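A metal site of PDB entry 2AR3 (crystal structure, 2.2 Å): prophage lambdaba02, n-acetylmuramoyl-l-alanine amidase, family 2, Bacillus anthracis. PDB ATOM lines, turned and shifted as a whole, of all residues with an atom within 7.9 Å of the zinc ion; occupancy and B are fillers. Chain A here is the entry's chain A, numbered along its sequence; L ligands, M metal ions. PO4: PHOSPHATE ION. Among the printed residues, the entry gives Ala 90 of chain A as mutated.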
ATOM      1  N   THR A  27      -7.181  24.001   2.506  1.00  0.00           N
ATOM      2  CA  THR A  27      -6.103  23.134   2.008  1.00  0.00           C
ATOM      3  C   THR A  27      -5.713  22.149   3.091  1.00  0.00           C
ATOM      4  O   THR A  27      -5.408  22.557   4.196  1.00  0.00           O
ATOM      5  CB  THR A  27      -4.857  23.940   1.630  1.00  0.00           C
ATOM      6  OG1 THR A  27      -5.188  24.891   0.593  1.00  0.00           O
ATOM      7  CG2 THR A  27      -3.705  22.977   1.158  1.00  0.00           C
ATOM      8  N   VAL A  28      -5.732  20.861   2.788  1.00  0.00           N
ATOM      9  CA  VAL A  28      -5.377  19.865   3.786  1.00  0.00           C
ATOM     10  C   VAL A  28      -3.947  19.360   3.620  1.00  0.00           C
ATOM     11  O   VAL A  28      -3.525  19.047   2.505  1.00  0.00           O
ATOM     12  CB  VAL A  28      -6.307  18.637   3.719  1.00  0.00           C
ATOM     13  CG1 VAL A  28      -5.894  17.640   4.781  1.00  0.00           C
ATOM     14  CG2 VAL A  28      -7.763  19.076   3.925  1.00  0.00           C
ATOM     15  N   HIS A  29      -3.232  19.273   4.733  1.00  0.00           N
ATOM     16  CA  HIS A  29      -1.858  18.816   4.714  1.00  0.00           C
ATOM     17  C   HIS A  29      -1.655  17.639   5.666  1.00  0.00           C
ATOM     18  O   HIS A  29      -2.551  17.253   6.436  1.00  0.00           O
ATOM     19  CB  HIS A  29      -0.902  19.941   5.168  1.00  0.00           C
ATOM     20  CG  HIS A  29      -1.082  21.250   4.461  1.00  0.00           C
ATOM     21  ND1 HIS A  29      -0.266  21.673   3.442  1.00  0.00           N
ATOM     22  CD2 HIS A  29      -1.965  22.257   4.682  1.00  0.00           C
ATOM     23  CE1 HIS A  29      -0.616  22.889   3.066  1.00  0.00           C
ATOM     24  NE2 HIS A  29      -1.645  23.261   3.793  1.00  0.00           N
ATOM     25  N   ASN A  30      -0.452  17.072   5.604  1.00  0.00           N
ATOM     26  CA  ASN A  30      -0.005  16.002   6.478  1.00  0.00           C
ATOM     27  C   ASN A  30       1.297  16.633   6.952  1.00  0.00           C
ATOM     28  O   ASN A  30       2.032  17.234   6.154  1.00  0.00           O
ATOM     29  CB  ASN A  30       0.279  14.692   5.712  1.00  0.00           C
ATOM     30  CG  ASN A  30      -0.907  13.736   5.685  1.00  0.00           C
ATOM     31  OD1 ASN A  30      -0.840  12.674   5.084  1.00  0.00           O
ATOM     32  ND2 ASN A  30      -2.007  14.099   6.354  1.00  0.00           N
ATOM     33  N   THR A  31       1.585  16.529   8.243  1.00  0.00           N
ATOM     34  CA  THR A  31       2.799  17.108   8.791  1.00  0.00           C
ATOM     35  C   THR A  31       4.041  16.249   8.568  1.00  0.00           C
ATOM     36  O   THR A  31       5.152  16.720   8.759  1.00  0.00           O
ATOM     37  CB  THR A  31       2.654  17.306  10.311  1.00  0.00           C
ATOM     38  OG1 THR A  31       2.607  16.012  10.933  1.00  0.00           O
ATOM     39  CG2 THR A  31       1.365  18.076  10.644  1.00  0.00           C
ATOM     40  N   TYR A  32       3.843  14.988   8.193  1.00  0.00           N
ATOM     41  CA  TYR A  32       4.970  14.068   7.986  1.00  0.00           C
ATOM     42  C   TYR A  32       5.805  14.095   9.262  1.00  0.00           C
ATOM     43  O   TYR A  32       7.035  14.134   9.201  1.00  0.00           O
ATOM     44  CB  TYR A  32       5.836  14.512   6.798  1.00  0.00           C
ATOM     45  CG  TYR A  32       6.886  13.481   6.361  1.00  0.00           C
ATOM     46  CD1 TYR A  32       6.501  12.224   5.888  1.00  0.00           C
ATOM     47  CD2 TYR A  32       8.257  13.777   6.400  1.00  0.00           C
ATOM     48  CE1 TYR A  32       7.442  11.282   5.452  1.00  0.00           C
ATOM     49  CE2 TYR A  32       9.206  12.856   5.966  1.00  0.00           C
ATOM     50  CZ  TYR A  32       8.794  11.609   5.501  1.00  0.00           C
ATOM     51  OH  TYR A  32       9.725  10.689   5.080  1.00  0.00           O
ATOM     52  N   ALA A  74       1.925  27.969   3.679  1.00  0.00           N
ATOM     53  CA  ALA A  74       1.965  26.511   3.777  1.00  0.00           C
ATOM     54  C   ALA A  74       1.767  25.785   2.446  1.00  0.00           C
ATOM     55  O   ALA A  74       1.929  24.560   2.376  1.00  0.00           O
ATOM     56  CB  ALA A  74       0.890  26.059   4.778  1.00  0.00           C
ATOM     57  N   CYS A  75       1.422  26.523   1.403  1.00  0.00           N
ATOM     58  CA  CYS A  75       1.159  25.910   0.094  1.00  0.00           C
ATOM     59  C   CYS A  75       2.314  25.979  -0.913  1.00  0.00           C
ATOM     60  O   CYS A  75       2.231  25.406  -2.009  1.00  0.00           O
ATOM     61  CB  CYS A  75      -0.112  26.534  -0.497  1.00  0.00           C
ATOM     62  SG  CYS A  75      -1.591  26.325   0.574  1.00  0.00           S
ATOM     63  N   GLY A  76       3.374  26.702  -0.552  1.00  0.00           N
ATOM     64  CA  GLY A  76       4.527  26.818  -1.429  1.00  0.00           C
ATOM     65  C   GLY A  76       4.252  27.353  -2.820  1.00  0.00           C
ATOM     66  O   GLY A  76       5.054  27.165  -3.731  1.00  0.00           O
ATOM     67  N   SER A  88      -5.169  26.618   5.911  1.00  0.00           N
ATOM     68  CA  SER A  88      -4.462  25.360   5.968  1.00  0.00           C
ATOM     69  C   SER A  88      -4.712  24.544   7.222  1.00  0.00           C
ATOM     70  O   SER A  88      -4.565  25.031   8.339  1.00  0.00           O
ATOM     71  CB  SER A  88      -2.963  25.591   5.787  1.00  0.00           C
ATOM     72  OG  SER A  88      -2.658  25.798   4.416  1.00  0.00           O
ATOM     73  N   VAL A  89      -5.086  23.291   7.015  1.00  0.00           N
ATOM     74  CA  VAL A  89      -5.341  22.373   8.096  1.00  0.00           C
ATOM     75  C   VAL A  89      -4.262  21.299   8.030  1.00  0.00           C
ATOM     76  O   VAL A  89      -4.088  20.638   6.997  1.00  0.00           O
ATOM     77  CB  VAL A  89      -6.726  21.730   7.943  1.00  0.00           C
ATOM     78  CG1 VAL A  89      -6.956  20.668   8.998  1.00  0.00           C
ATOM     79  CG2 VAL A  89      -7.789  22.821   8.062  1.00  0.00           C
ATOM     80  N   ALA A  90      -3.527  21.118   9.119  1.00  0.00           N
ATOM     81  CA  ALA A  90      -2.468  20.116   9.147  1.00  0.00           C
ATOM     82  C   ALA A  90      -2.820  18.978  10.102  1.00  0.00           C
ATOM     83  O   ALA A  90      -3.129  19.200  11.275  1.00  0.00           O
ATOM     84  CB  ALA A  90      -1.156  20.760   9.557  1.00  0.00           C
ATOM     85  N   THR A 128      -5.923  19.776  -1.721  1.00  0.00           N
ATOM     86  CA  THR A 128      -4.719  19.174  -1.178  1.00  0.00           C
ATOM     87  C   THR A 128      -3.621  20.184  -1.429  1.00  0.00           C
ATOM     88  O   THR A 128      -3.778  21.073  -2.268  1.00  0.00           O
ATOM     89  CB  THR A 128      -4.332  17.905  -1.953  1.00  0.00           C
ATOM     90  OG1 THR A 128      -4.035  18.275  -3.312  1.00  0.00           O
ATOM     91  CG2 THR A 128      -5.455  16.866  -1.937  1.00  0.00           C
ATOM     92  N   HIS A 129      -2.504  20.037  -0.701  1.00  0.00           N
ATOM     93  CA  HIS A 129      -1.351  20.925  -0.887  1.00  0.00           C
ATOM     94  C   HIS A 129      -0.807  20.659  -2.295  1.00  0.00           C
ATOM     95  O   HIS A 129      -0.447  21.582  -3.030  1.00  0.00           O
ATOM     96  CB  HIS A 129      -0.273  20.626   0.166  1.00  0.00           C
ATOM     97  CG  HIS A 129       0.989  21.431   0.023  1.00  0.00           C
ATOM     98  ND1 HIS A 129       2.023  21.345   0.928  1.00  0.00           N
ATOM     99  CD2 HIS A 129       1.402  22.297  -0.938  1.00  0.00           C
ATOM    100  CE1 HIS A 129       3.024  22.113   0.530  1.00  0.00           C
ATOM    101  NE2 HIS A 129       2.679  22.700  -0.597  1.00  0.00           N
ATOM    102  N   GLN A 130      -0.772  19.393  -2.664  1.00  0.00           N
ATOM    103  CA  GLN A 130      -0.276  18.997  -3.979  1.00  0.00           C
ATOM    104  C   GLN A 130      -0.946  19.744  -5.134  1.00  0.00           C
ATOM    105  O   GLN A 130      -0.276  20.111  -6.098  1.00  0.00           O
ATOM    106  CB  GLN A 130      -0.474  17.495  -4.180  1.00  0.00           C
ATOM    107  CG  GLN A 130      -0.019  16.963  -5.525  1.00  0.00           C
ATOM    108  CD  GLN A 130      -0.272  15.471  -5.642  1.00  0.00           C
ATOM    109  OE1 GLN A 130      -1.390  15.002  -5.418  1.00  0.00           O
ATOM    110  NE2 GLN A 130       0.776  14.724  -5.989  1.00  0.00           N
ATOM    111  N   SER A 133       0.905  23.355  -5.511  1.00  0.00           N
ATOM    112  CA  SER A 133       2.319  23.487  -5.906  1.00  0.00           C
ATOM    113  C   SER A 133       3.007  22.214  -6.366  1.00  0.00           C
ATOM    114  O   SER A 133       4.155  22.261  -6.820  1.00  0.00           O
ATOM    115  CB  SER A 133       3.111  24.092  -4.752  1.00  0.00           C
ATOM    116  OG  SER A 133       3.051  23.235  -3.622  1.00  0.00           O
ATOM    117  N   LYS A 135       3.764  19.541  -4.414  1.00  0.00           N
ATOM    118  CA  LYS A 135       4.381  18.773  -3.329  1.00  0.00           C
ATOM    119  C   LYS A 135       3.511  17.556  -3.004  1.00  0.00           C
ATOM    120  O   LYS A 135       2.285  17.619  -3.101  1.00  0.00           O
ATOM    121  CB  LYS A 135       4.546  19.631  -2.065  1.00  0.00           C
ATOM    122  CG  LYS A 135       5.421  18.970  -0.973  1.00  0.00           C
ATOM    123  CD  LYS A 135       5.706  19.890   0.199  1.00  0.00           C
ATOM    124  CE  LYS A 135       6.706  19.247   1.173  1.00  0.00           C
ATOM    125  NZ  LYS A 135       7.130  20.180   2.268  1.00  0.00           N
ATOM    126  N   TYR A 136       4.145  16.460  -2.608  1.00  0.00           N
ATOM    127  CA  TYR A 136       3.427  15.247  -2.274  1.00  0.00           C
ATOM    128  C   TYR A 136       2.865  15.354  -0.846  1.00  0.00           C
ATOM    129  O   TYR A 136       3.356  14.703   0.070  1.00  0.00           O
ATOM    130  CB  TYR A 136       4.376  14.032  -2.392  1.00  0.00           C
ATOM    131  CG  TYR A 136       3.664  12.682  -2.423  1.00  0.00           C
ATOM    132  CD1 TYR A 136       2.783  12.363  -3.451  1.00  0.00           C
ATOM    133  CD2 TYR A 136       3.869  11.746  -1.407  1.00  0.00           C
ATOM    134  CE1 TYR A 136       2.112  11.146  -3.476  1.00  0.00           C
ATOM    135  CE2 TYR A 136       3.203  10.511  -1.416  1.00  0.00           C
ATOM    136  CZ  TYR A 136       2.327  10.220  -2.456  1.00  0.00           C
ATOM    137  OH  TYR A 136       1.669   9.016  -2.465  1.00  0.00           O
ATOM    138  N   CYS A 137       1.843  16.187  -0.699  1.00  0.00           N
ATOM    139  CA  CYS A 137       1.163  16.432   0.562  1.00  0.00           C
ATOM    140  C   CYS A 137      -0.360  16.579   0.303  1.00  0.00           C
ATOM    141  O   CYS A 137      -0.758  17.281  -0.627  1.00  0.00           O
ATOM    142  CB  CYS A 137       1.703  17.709   1.169  1.00  0.00           C
ATOM    143  SG  CYS A 137       0.582  18.210   2.456  1.00  0.00           S
ATOM    144  N   PRO A 138      -1.228  15.916   1.108  1.00  0.00           N
ATOM    145  CA  PRO A 138      -0.930  15.037   2.245  1.00  0.00           C
ATOM    146  C   PRO A 138      -0.409  13.664   1.822  1.00  0.00           C
ATOM    147  O   PRO A 138      -1.152  12.819   1.322  1.00  0.00           O
ATOM    148  CB  PRO A 138      -2.271  14.959   2.976  1.00  0.00           C
ATOM    149  CG  PRO A 138      -3.249  15.022   1.877  1.00  0.00           C
ATOM    150  CD  PRO A 138      -2.678  16.042   0.912  1.00  0.00           C
ATOM    151  N   HIS A 139       0.882  13.459   2.059  1.00  0.00           N
ATOM    152  CA  HIS A 139       1.587  12.238   1.692  1.00  0.00           C
ATOM    153  C   HIS A 139       0.906  10.929   2.057  1.00  0.00           C
ATOM    154  O   HIS A 139       0.802  10.044   1.211  1.00  0.00           O
ATOM    155  CB  HIS A 139       2.996  12.251   2.281  1.00  0.00           C
ATOM    156  CG  HIS A 139       3.065  11.931   3.732  1.00  0.00           C
ATOM    157  ND1 HIS A 139       3.054  10.631   4.215  1.00  0.00           N
ATOM    158  CD2 HIS A 139       3.151  12.726   4.828  1.00  0.00           C
ATOM    159  CE1 HIS A 139       3.129  10.646   5.530  1.00  0.00           C
ATOM    160  NE2 HIS A 139       3.193  11.907   5.927  1.00  0.00           N
HETATM  161  P   PO4 L   1       4.096  20.364   4.325  1.00  0.00           P
HETATM  162  O1  PO4 L   1       5.442  20.895   4.709  1.00  0.00           O
HETATM  163  O2  PO4 L   1       4.197  19.658   3.022  1.00  0.00           O
HETATM  164  O3  PO4 L   1       3.631  19.416   5.359  1.00  0.00           O
HETATM  165  O4  PO4 L   1       3.137  21.489   4.211  1.00  0.00           O
HETATM  166 ZN    ZN M   1       1.435  20.369   2.964  1.00  0.00          ZN
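The zinc ion is bound by ND1 of His 29 (2.2 Å), ND1 of His 129 (2.3 Å), SG of Cys 137 (2.4 Å) and O4 of the ligand (2.4 Å).
The backbone NH of His 29 lies within hydrogen-bond range of the backbone carbonyl oxygen of Val 89 (2.8 Å). NE2 of His 29 is in hydrogen-bond range of OG of Ser 88 (2.8 Å). The backbone carbonyl oxygen of Cys 75 lies within hydrogen-bond range of a ring nitrogen (NE2) of His 129 (3.1 Å). NE2 of His 129 lies within hydrogen-bond range of OG of Ser 133. SG of Cys 137 sits close to N of Asn 30 (3.5 Å). The backbone carbonyl oxygen of Cys 137 lies within hydrogen-bond range of the backbone NH of Gln 130 (2.9 Å).
Of the 21 residues printed, 3 come within 4 Å of the zinc ion. The nearest printed residue that does not touch the zinc ion is Ala 74 (4.3 Å).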
